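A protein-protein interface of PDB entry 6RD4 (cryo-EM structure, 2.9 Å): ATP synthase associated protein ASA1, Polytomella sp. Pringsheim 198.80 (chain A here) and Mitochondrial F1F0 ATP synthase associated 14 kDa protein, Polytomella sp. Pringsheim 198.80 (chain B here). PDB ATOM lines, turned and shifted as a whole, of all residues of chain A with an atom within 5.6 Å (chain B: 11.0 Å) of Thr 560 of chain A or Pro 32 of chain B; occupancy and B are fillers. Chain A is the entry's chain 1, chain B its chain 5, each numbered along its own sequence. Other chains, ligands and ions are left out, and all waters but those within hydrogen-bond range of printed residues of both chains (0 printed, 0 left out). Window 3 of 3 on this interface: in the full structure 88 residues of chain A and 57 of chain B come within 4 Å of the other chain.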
ATOM      1  N   ILE A 556      25.578  20.181  37.160  1.00  0.00           N
ATOM      2  CA  ILE A 556      25.555  19.603  35.825  1.00  0.00           C
ATOM      3  C   ILE A 556      26.936  19.654  35.206  1.00  0.00           C
ATOM      4  O   ILE A 556      27.398  18.682  34.610  1.00  0.00           O
ATOM      5  CB  ILE A 556      24.519  20.334  34.961  1.00  0.00           C
ATOM      6  CG1 ILE A 556      23.117  19.861  35.274  1.00  0.00           C
ATOM      7  CG2 ILE A 556      24.757  20.115  33.538  1.00  0.00           C
ATOM      8  CD1 ILE A 556      22.106  20.756  34.738  1.00  0.00           C
ATOM      9  N   ASP A 557      27.634  20.769  35.377  1.00  0.00           N
ATOM     10  CA  ASP A 557      28.994  20.911  34.891  1.00  0.00           C
ATOM     11  C   ASP A 557      29.971  20.010  35.600  1.00  0.00           C
ATOM     12  O   ASP A 557      31.059  19.794  35.085  1.00  0.00           O
ATOM     13  CB  ASP A 557      29.479  22.332  35.072  1.00  0.00           C
ATOM     14  CG  ASP A 557      28.820  23.282  34.155  1.00  0.00           C
ATOM     15  OD1 ASP A 557      27.946  22.853  33.397  1.00  0.00           O
ATOM     16  OD2 ASP A 557      29.180  24.465  34.185  1.00  0.00           O
ATOM     17  N   TRP A 558      29.652  19.535  36.790  1.00  0.00           N
ATOM     18  CA  TRP A 558      30.536  18.587  37.443  1.00  0.00           C
ATOM     19  C   TRP A 558      30.485  17.245  36.753  1.00  0.00           C
ATOM     20  O   TRP A 558      31.484  16.540  36.702  1.00  0.00           O
ATOM     21  CB  TRP A 558      30.179  18.440  38.914  1.00  0.00           C
ATOM     22  CG  TRP A 558      31.126  17.588  39.659  1.00  0.00           C
ATOM     23  CD1 TRP A 558      32.222  17.989  40.305  1.00  0.00           C
ATOM     24  CD2 TRP A 558      31.059  16.172  39.821  1.00  0.00           C
ATOM     25  NE1 TRP A 558      32.856  16.923  40.861  1.00  0.00           N
ATOM     26  CE2 TRP A 558      32.144  15.796  40.576  1.00  0.00           C
ATOM     27  CE3 TRP A 558      30.177  15.190  39.393  1.00  0.00           C
ATOM     28  CZ2 TRP A 558      32.388  14.498  40.892  1.00  0.00           C
ATOM     29  CZ3 TRP A 558      30.416  13.927  39.705  1.00  0.00           C
ATOM     30  CH2 TRP A 558      31.503  13.576  40.447  1.00  0.00           C
ATOM     31  N   GLU A 559      29.331  16.862  36.237  1.00  0.00           N
ATOM     32  CA  GLU A 559      29.236  15.594  35.541  1.00  0.00           C
ATOM     33  C   GLU A 559      29.943  15.643  34.205  1.00  0.00           C
ATOM     34  O   GLU A 559      30.513  14.648  33.773  1.00  0.00           O
ATOM     35  CB  GLU A 559      27.789  15.230  35.342  1.00  0.00           C
ATOM     36  CG  GLU A 559      27.004  15.328  36.560  1.00  0.00           C
ATOM     37  CD  GLU A 559      25.701  14.635  36.435  1.00  0.00           C
ATOM     38  OE1 GLU A 559      25.566  13.813  35.528  1.00  0.00           O
ATOM     39  OE2 GLU A 559      24.800  14.909  37.233  1.00  0.00           O
ATOM     40  N   THR A 560      29.895  16.775  33.519  1.00  0.00           N
ATOM     41  CA  THR A 560      30.618  16.886  32.265  1.00  0.00           C
ATOM     42  C   THR A 560      32.113  16.937  32.504  1.00  0.00           C
ATOM     43  O   THR A 560      32.878  16.351  31.747  1.00  0.00           O
ATOM     44  CB  THR A 560      30.157  18.113  31.497  1.00  0.00           C
ATOM     45  OG1 THR A 560      28.735  18.137  31.474  1.00  0.00           O
ATOM     46  CG2 THR A 560      30.620  18.060  30.111  1.00  0.00           C
ATOM     47  N   THR A 561      32.543  17.608  33.565  1.00  0.00           N
ATOM     48  CA  THR A 561      33.965  17.707  33.856  1.00  0.00           C
ATOM     49  C   THR A 561      34.530  16.372  34.275  1.00  0.00           C
ATOM     50  O   THR A 561      35.616  15.984  33.848  1.00  0.00           O
ATOM     51  CB  THR A 561      34.187  18.733  34.945  1.00  0.00           C
ATOM     52  OG1 THR A 561      33.619  19.969  34.533  1.00  0.00           O
ATOM     53  CG2 THR A 561      35.620  18.945  35.195  1.00  0.00           C
ATOM     54  N   ASN A 562      33.783  15.634  35.076  1.00  0.00           N
ATOM     55  CA  ASN A 562      34.228  14.365  35.614  1.00  0.00           C
ATOM     56  C   ASN A 562      33.687  13.194  34.845  1.00  0.00           C
ATOM     57  O   ASN A 562      33.380  12.169  35.443  1.00  0.00           O
ATOM     58  CB  ASN A 562      33.841  14.270  37.069  1.00  0.00           C
ATOM     59  CG  ASN A 562      34.543  15.273  37.872  1.00  0.00           C
ATOM     60  OD1 ASN A 562      34.112  16.396  37.963  1.00  0.00           O
ATOM     61  ND2 ASN A 562      35.669  14.906  38.420  1.00  0.00           N
ATOM     62  N   ALA A 563      33.510  13.367  33.544  1.00  0.00           N
ATOM     63  CA  ALA A 563      33.327  12.310  32.564  1.00  0.00           C
ATOM     64  C   ALA A 563      32.097  11.471  32.808  1.00  0.00           C
ATOM     65  O   ALA A 563      32.044  10.318  32.401  1.00  0.00           O
ATOM     66  CB  ALA A 563      34.557  11.416  32.497  1.00  0.00           C
ATOM     67  N   LEU A 564      31.108  12.017  33.485  1.00  0.00           N
ATOM     68  CA  LEU A 564      29.857  11.336  33.743  1.00  0.00           C
ATOM     69  C   LEU A 564      28.719  12.048  33.049  1.00  0.00           C
ATOM     70  O   LEU A 564      27.624  12.141  33.582  1.00  0.00           O
ATOM     71  CB  LEU A 564      29.562  11.266  35.229  1.00  0.00           C
ATOM     72  CG  LEU A 564      30.504  10.611  36.212  1.00  0.00           C
ATOM     73  CD1 LEU A 564      30.119  11.097  37.547  1.00  0.00           C
ATOM     74  CD2 LEU A 564      30.325   9.148  36.154  1.00  0.00           C
ATOM     75  N   GLU A 565      28.961  12.559  31.844  1.00  0.00           N
ATOM     76  CA  GLU A 565      27.922  13.286  31.137  1.00  0.00           C
ATOM     77  C   GLU A 565      26.811  12.383  30.648  1.00  0.00           C
ATOM     78  O   GLU A 565      25.776  12.876  30.211  1.00  0.00           O
ATOM     79  CB  GLU A 565      28.501  14.053  29.957  1.00  0.00           C
ATOM     80  CG  GLU A 565      28.988  13.185  28.852  1.00  0.00           C
ATOM     81  CD  GLU A 565      30.448  12.889  28.959  1.00  0.00           C
ATOM     82  OE1 GLU A 565      31.051  13.270  29.971  1.00  0.00           O
ATOM     83  OE2 GLU A 565      31.001  12.259  28.043  1.00  0.00           O
ATOM     84  N   VAL B  22      36.934  18.113  16.059  1.00  0.00           N
ATOM     85  CA  VAL B  22      35.554  17.742  16.322  1.00  0.00           C
ATOM     86  C   VAL B  22      35.440  17.080  17.682  1.00  0.00           C
ATOM     87  O   VAL B  22      34.448  17.251  18.378  1.00  0.00           O
ATOM     88  CB  VAL B  22      35.025  16.858  15.184  1.00  0.00           C
ATOM     89  CG1 VAL B  22      33.649  16.408  15.436  1.00  0.00           C
ATOM     90  CG2 VAL B  22      35.027  17.632  13.933  1.00  0.00           C
ATOM     91  N   LEU B  23      36.475  16.382  18.120  1.00  0.00           N
ATOM     92  CA  LEU B  23      36.458  15.840  19.467  1.00  0.00           C
ATOM     93  C   LEU B  23      36.556  16.932  20.503  1.00  0.00           C
ATOM     94  O   LEU B  23      35.833  16.905  21.493  1.00  0.00           O
ATOM     95  CB  LEU B  23      37.593  14.861  19.661  1.00  0.00           C
ATOM     96  CG  LEU B  23      37.633  14.216  21.018  1.00  0.00           C
ATOM     97  CD1 LEU B  23      36.472  13.330  21.120  1.00  0.00           C
ATOM     98  CD2 LEU B  23      38.875  13.447  21.093  1.00  0.00           C
ATOM     99  N   TRP B  24      37.430  17.903  20.290  1.00  0.00           N
ATOM    100  CA  TRP B  24      37.522  19.027  21.206  1.00  0.00           C
ATOM    101  C   TRP B  24      36.251  19.842  21.191  1.00  0.00           C
ATOM    102  O   TRP B  24      35.736  20.192  22.240  1.00  0.00           O
ATOM    103  CB  TRP B  24      38.712  19.910  20.865  1.00  0.00           C
ATOM    104  CG  TRP B  24      38.669  21.196  21.575  1.00  0.00           C
ATOM    105  CD1 TRP B  24      39.080  21.438  22.824  1.00  0.00           C
ATOM    106  CD2 TRP B  24      38.173  22.429  21.073  1.00  0.00           C
ATOM    107  NE1 TRP B  24      38.863  22.737  23.150  1.00  0.00           N
ATOM    108  CE2 TRP B  24      38.295  23.364  22.081  1.00  0.00           C
ATOM    109  CE3 TRP B  24      37.607  22.821  19.868  1.00  0.00           C
ATOM    110  CZ2 TRP B  24      37.892  24.658  21.922  1.00  0.00           C
ATOM    111  CZ3 TRP B  24      37.211  24.095  19.720  1.00  0.00           C
ATOM    112  CH2 TRP B  24      37.351  24.999  20.732  1.00  0.00           C
ATOM    113  N   HIS B  25      35.718  20.141  20.016  1.00  0.00           N
ATOM    114  CA  HIS B  25      34.540  20.987  19.940  1.00  0.00           C
ATOM    115  C   HIS B  25      33.319  20.327  20.521  1.00  0.00           C
ATOM    116  O   HIS B  25      32.498  20.996  21.130  1.00  0.00           O
ATOM    117  CB  HIS B  25      34.252  21.358  18.515  1.00  0.00           C
ATOM    118  CG  HIS B  25      33.367  22.538  18.398  1.00  0.00           C
ATOM    119  ND1 HIS B  25      32.025  22.438  18.149  1.00  0.00           N
ATOM    120  CD2 HIS B  25      33.625  23.850  18.552  1.00  0.00           C
ATOM    121  CE1 HIS B  25      31.497  23.643  18.126  1.00  0.00           C
ATOM    122  NE2 HIS B  25      32.447  24.517  18.373  1.00  0.00           N
ATOM    123  N   LEU B  26      33.196  19.026  20.379  1.00  0.00           N
ATOM    124  CA  LEU B  26      32.086  18.326  20.985  1.00  0.00           C
ATOM    125  C   LEU B  26      32.222  18.292  22.494  1.00  0.00           C
ATOM    126  O   LEU B  26      31.281  18.618  23.207  1.00  0.00           O
ATOM    127  CB  LEU B  26      32.027  16.928  20.426  1.00  0.00           C
ATOM    128  CG  LEU B  26      30.915  16.002  20.770  1.00  0.00           C
ATOM    129  CD1 LEU B  26      29.753  16.369  19.944  1.00  0.00           C
ATOM    130  CD2 LEU B  26      31.440  14.686  20.411  1.00  0.00           C
ATOM    131  N   ASP B  27      33.393  17.926  22.999  1.00  0.00           N
ATOM    132  CA  ASP B  27      33.584  17.754  24.431  1.00  0.00           C
ATOM    133  C   ASP B  27      33.542  19.046  25.196  1.00  0.00           C
ATOM    134  O   ASP B  27      33.217  19.047  26.379  1.00  0.00           O
ATOM    135  CB  ASP B  27      34.925  17.149  24.714  1.00  0.00           C
ATOM    136  CG  ASP B  27      34.890  15.695  24.837  1.00  0.00           C
ATOM    137  OD1 ASP B  27      33.848  15.143  25.210  1.00  0.00           O
ATOM    138  OD2 ASP B  27      35.947  15.095  24.633  1.00  0.00           O
ATOM    139  N   THR B  28      33.934  20.131  24.571  1.00  0.00           N
ATOM    140  CA  THR B  28      34.117  21.399  25.240  1.00  0.00           C
ATOM    141  C   THR B  28      32.968  22.352  24.977  1.00  0.00           C
ATOM    142  O   THR B  28      32.466  22.977  25.896  1.00  0.00           O
ATOM    143  CB  THR B  28      35.442  21.989  24.790  1.00  0.00           C
ATOM    144  OG1 THR B  28      36.504  21.287  25.415  1.00  0.00           O
ATOM    145  CG2 THR B  28      35.563  23.390  25.102  1.00  0.00           C
ATOM    146  N   GLN B  29      32.507  22.441  23.743  1.00  0.00           N
ATOM    147  CA  GLN B  29      31.493  23.410  23.384  1.00  0.00           C
ATOM    148  C   GLN B  29      30.116  22.808  23.218  1.00  0.00           C
ATOM    149  O   GLN B  29      29.150  23.361  23.731  1.00  0.00           O
ATOM    150  CB  GLN B  29      31.898  24.134  22.109  1.00  0.00           C
ATOM    151  CG  GLN B  29      33.332  24.556  22.100  1.00  0.00           C
ATOM    152  CD  GLN B  29      33.568  25.771  22.912  1.00  0.00           C
ATOM    153  OE1 GLN B  29      34.664  26.016  23.389  1.00  0.00           O
ATOM    154  NE2 GLN B  29      32.533  26.570  23.081  1.00  0.00           N
ATOM    155  N   LEU B  30      29.994  21.695  22.516  1.00  0.00           N
ATOM    156  CA  LEU B  30      28.667  21.145  22.284  1.00  0.00           C
ATOM    157  C   LEU B  30      28.139  20.401  23.493  1.00  0.00           C
ATOM    158  O   LEU B  30      27.062  20.718  23.979  1.00  0.00           O
ATOM    159  CB  LEU B  30      28.675  20.238  21.071  1.00  0.00           C
ATOM    160  CG  LEU B  30      28.973  20.929  19.764  1.00  0.00           C
ATOM    161  CD1 LEU B  30      28.778  19.952  18.678  1.00  0.00           C
ATOM    162  CD2 LEU B  30      28.085  22.099  19.567  1.00  0.00           C
ATOM    163  N   LEU B  31      28.880  19.424  24.007  1.00  0.00           N
ATOM    164  CA  LEU B  31      28.337  18.578  25.063  1.00  0.00           C
ATOM    165  C   LEU B  31      28.125  19.242  26.416  1.00  0.00           C
ATOM    166  O   LEU B  31      27.293  18.723  27.172  1.00  0.00           O
ATOM    167  CB  LEU B  31      29.208  17.345  25.283  1.00  0.00           C
ATOM    168  CG  LEU B  31      28.978  16.064  24.518  1.00  0.00           C
ATOM    169  CD1 LEU B  31      29.934  15.061  25.055  1.00  0.00           C
ATOM    170  CD2 LEU B  31      27.577  15.631  24.727  1.00  0.00           C
ATOM    171  N   PRO B  32      28.841  20.287  26.822  1.00  0.00           N
ATOM    172  CA  PRO B  32      28.363  21.056  27.962  1.00  0.00           C
ATOM    173  C   PRO B  32      27.032  21.726  27.749  1.00  0.00           C
ATOM    174  O   PRO B  32      26.232  21.767  28.675  1.00  0.00           O
ATOM    175  CB  PRO B  32      29.489  22.056  28.153  1.00  0.00           C
ATOM    176  CG  PRO B  32      30.608  21.273  27.896  1.00  0.00           C
ATOM    177  CD  PRO B  32      30.293  20.464  26.733  1.00  0.00           C
ATOM    178  N   THR B  33      26.762  22.237  26.566  1.00  0.00           N
ATOM    179  CA  THR B  33      25.480  22.831  26.241  1.00  0.00           C
ATOM    180  C   THR B  33      24.375  21.796  26.109  1.00  0.00           C
ATOM    181  O   THR B  33      23.239  22.065  26.503  1.00  0.00           O
ATOM    182  CB  THR B  33      25.638  23.604  24.948  1.00  0.00           C
ATOM    183  OG1 THR B  33      26.683  24.561  25.113  1.00  0.00           O
ATOM    184  CG2 THR B  33      24.402  24.294  24.579  1.00  0.00           C
ATOM    185  N   ILE B  34      24.685  20.626  25.546  1.00  0.00           N
ATOM    186  CA  ILE B  34      23.721  19.534  25.451  1.00  0.00           C
ATOM    187  C   ILE B  34      23.260  19.136  26.832  1.00  0.00           C
ATOM    188  O   ILE B  34      22.068  19.059  27.104  1.00  0.00           O
ATOM    189  CB  ILE B  34      24.334  18.321  24.732  1.00  0.00           C
ATOM    190  CG1 ILE B  34      24.717  18.607  23.295  1.00  0.00           C
ATOM    191  CG2 ILE B  34      23.429  17.143  24.794  1.00  0.00           C
ATOM    192  CD1 ILE B  34      23.689  19.124  22.509  1.00  0.00           C
ATOM    193  N   MET B  35      24.201  18.909  27.730  1.00  0.00           N
ATOM    194  CA  MET B  35      23.898  18.380  29.040  1.00  0.00           C
ATOM    195  C   MET B  35      23.377  19.429  29.988  1.00  0.00           C
ATOM    196  O   MET B  35      22.825  19.074  31.015  1.00  0.00           O
ATOM    197  CB  MET B  35      25.130  17.734  29.641  1.00  0.00           C
ATOM    198  CG  MET B  35      25.552  16.493  28.967  1.00  0.00           C
ATOM    199  SD  MET B  35      24.177  15.447  28.584  1.00  0.00           S
ATOM    200  CE  MET B  35      24.897  14.532  27.268  1.00  0.00           C
ATOM    201  N   ARG B  36      23.527  20.701  29.689  1.00  0.00           N
ATOM    202  CA  ARG B  36      22.954  21.697  30.566  1.00  0.00           C
ATOM    203  C   ARG B  36      21.466  21.778  30.375  1.00  0.00           C
ATOM    204  O   ARG B  36      20.736  22.099  31.306  1.00  0.00           O
ATOM    205  CB  ARG B  36      23.583  23.046  30.313  1.00  0.00           C
ATOM    206  CG  ARG B  36      24.729  23.325  31.178  1.00  0.00           C
ATOM    207  CD  ARG B  36      25.335  24.587  30.760  1.00  0.00           C
ATOM    208  NE  ARG B  36      26.601  24.808  31.416  1.00  0.00           N
ATOM    209  CZ  ARG B  36      27.084  26.009  31.647  1.00  0.00           C
ATOM    210  NH1 ARG B  36      28.235  26.153  32.261  1.00  0.00           N
ATOM    211  NH2 ARG B  36      26.388  27.060  31.277  1.00  0.00           N
ATOM    212  N   GLU B  37      20.996  21.503  29.185  1.00  0.00           N
ATOM    213  CA  GLU B  37      19.574  21.533  28.957  1.00  0.00           C
ATOM    214  C   GLU B  37      18.963  20.160  28.866  1.00  0.00           C
ATOM    215  O   GLU B  37      17.753  20.038  29.002  1.00  0.00           O
ATOM    216  CB  GLU B  37      19.272  22.326  27.710  1.00  0.00           C
ATOM    217  CG  GLU B  37      19.448  21.638  26.470  1.00  0.00           C
ATOM    218  CD  GLU B  37      18.979  22.496  25.350  1.00  0.00           C
ATOM    219  OE1 GLU B  37      19.653  23.495  25.067  1.00  0.00           O
ATOM    220  OE2 GLU B  37      17.919  22.198  24.768  1.00  0.00           O
ATOM    221  N   HIS B  38      19.757  19.120  28.693  1.00  0.00           N
ATOM    222  CA  HIS B  38      19.213  17.789  28.853  1.00  0.00           C
ATOM    223  C   HIS B  38      18.977  17.491  30.311  1.00  0.00           C
ATOM    224  O   HIS B  38      17.947  16.926  30.669  1.00  0.00           O
ATOM    225  CB  HIS B  38      20.146  16.756  28.249  1.00  0.00           C
ATOM    226  CG  HIS B  38      19.811  15.352  28.619  1.00  0.00           C
ATOM    227  ND1 HIS B  38      18.567  14.812  28.417  1.00  0.00           N
ATOM    228  CD2 HIS B  38      20.562  14.372  29.162  1.00  0.00           C
ATOM    229  CE1 HIS B  38      18.559  13.566  28.839  1.00  0.00           C
ATOM    230  NE2 HIS B  38      19.759  13.273  29.292  1.00  0.00           N
ATOM    231  N   LYS B  39      19.905  17.872  31.170  1.00  0.00           N
ATOM    232  CA  LYS B  39      19.825  17.528  32.573  1.00  0.00           C
ATOM    233  C   LYS B  39      19.102  18.548  33.421  1.00  0.00           C
ATOM    234  O   LYS B  39      18.868  18.272  34.584  1.00  0.00           O
ATOM    235  CB  LYS B  39      21.208  17.326  33.143  1.00  0.00           C
ATOM    236  CG  LYS B  39      21.888  16.173  32.560  1.00  0.00           C
ATOM    237  CD  LYS B  39      23.241  16.044  33.091  1.00  0.00           C
ATOM    238  CE  LYS B  39      23.806  14.763  32.643  1.00  0.00           C
ATOM    239  NZ  LYS B  39      25.182  14.741  33.067  1.00  0.00           N
ATOM    240  N   LEU B  40      18.760  19.717  32.912  1.00  0.00           N
ATOM    241  CA  LEU B  40      17.754  20.485  33.618  1.00  0.00           C
ATOM    242  C   LEU B  40      16.413  19.801  33.497  1.00  0.00           C
ATOM    243  O   LEU B  40      15.670  19.702  34.466  1.00  0.00           O
ATOM    244  CB  LEU B  40      17.676  21.903  33.082  1.00  0.00           C
ATOM    245  CG  LEU B  40      16.704  22.785  33.853  1.00  0.00           C
ATOM    246  CD1 LEU B  40      17.350  24.038  34.128  1.00  0.00           C
ATOM    247  CD2 LEU B  40      15.491  23.092  33.071  1.00  0.00           C
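The side-chain sulfur of Met 35 of chain B sits close to the backbone carbonyl oxygen of Glu 565 of chain A (3.4 Å). O of Glu 565 of chain A is in hydrogen-bond range of NZ of Lys 39 of chain B (3.5 Å). The side-chain amino group (NZ) of Lys 39 of chain B is in salt-bridge range of the side-chain carboxylate (OE1) of Glu 559 of chain A (2.7 Å). The guanidinium group (NH1) of Arg 36 of chain B lies within salt-bridge range of the side-chain carboxylate (OD2) of Asp 557 of chain A, at 2.7 Å.
The backbone carbonyl oxygen (O) of Glu 559 of chain A is in hydrogen-bond range of the backbone NH (N) of Glu 565 of chain A (3.2 Å). The side-chain hydroxyl (OG1) of Thr 561 of chain A sits at hydrogen-bond distance from the backbone carbonyl oxygen (O) of Asp 557 of chain A (2.6 Å). The backbone NH (N) of Leu 564 of chain A sits at hydrogen-bond distance from the backbone carbonyl oxygen (O) of Glu 559 of chain A, 2.7 Å away. The side-chain hydroxyl (OG1) of Thr 560 of chain A lies within hydrogen-bond range of the backbone carbonyl oxygen (O) of Ile 556 of chain A, 3.5 Å away.
Among the printed residues, pairs that only touch across the chains: Ile 556 of chain A with Met 35 of chain B, Ile 556 of chain A with Arg 36 of chain B, Ile 556 of chain A with Lys 39 of chain B, Ile 556 of chain A with Leu 40 of chain B, Thr 560 of chain A with Pro 32 of chain B and Leu 564 of chain A with Lys 39 of chain B.
Pro 32 of chain B touches one residue of chain A. No residue of chain B comes within 4 Å of Ala 563 of chain A. Printed residues of chain B within 4 Å of Glu 565 of chain A: Met 35 and Lys 39. Of the printed residues of chain B, Ile 556 of chain A touches Met 35, Arg 36, Lys 39 and Leu 40. Printed residues of chain A within 4 Å of Met 35 of chain B: Ile 556 (3.3 Å) and Glu 565 (3.4 Å). Of the printed residues of chain A, Lys 39 of chain B touches Ile 556, Glu 559, Leu 564 and Glu 565. Of the printed residues of chain B, Leu 564 of chain A touches Lys 39 (3.6 Å). The nearest residue of chain B that does not touch Thr 560 of chain A is Met 35 of chain B (4.1 Å).
Of the 10 printed residues of chain A, 6 touch a printed residue of chain B. Hydrophobic or aromatic side chains of chain A that line the printed part of chain B: Ile 556. Along chain A the printed residues that touch a printed residue of chain B span positions 556 to 565. Of the 19 printed residues of chain B, 5 touch a printed residue of chain A. Hydrophobic or aromatic side chains of chain B that line the printed part of chain A: Pro 32 and Met 35. Among the printed residues, 10 pairs touch across the chains.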
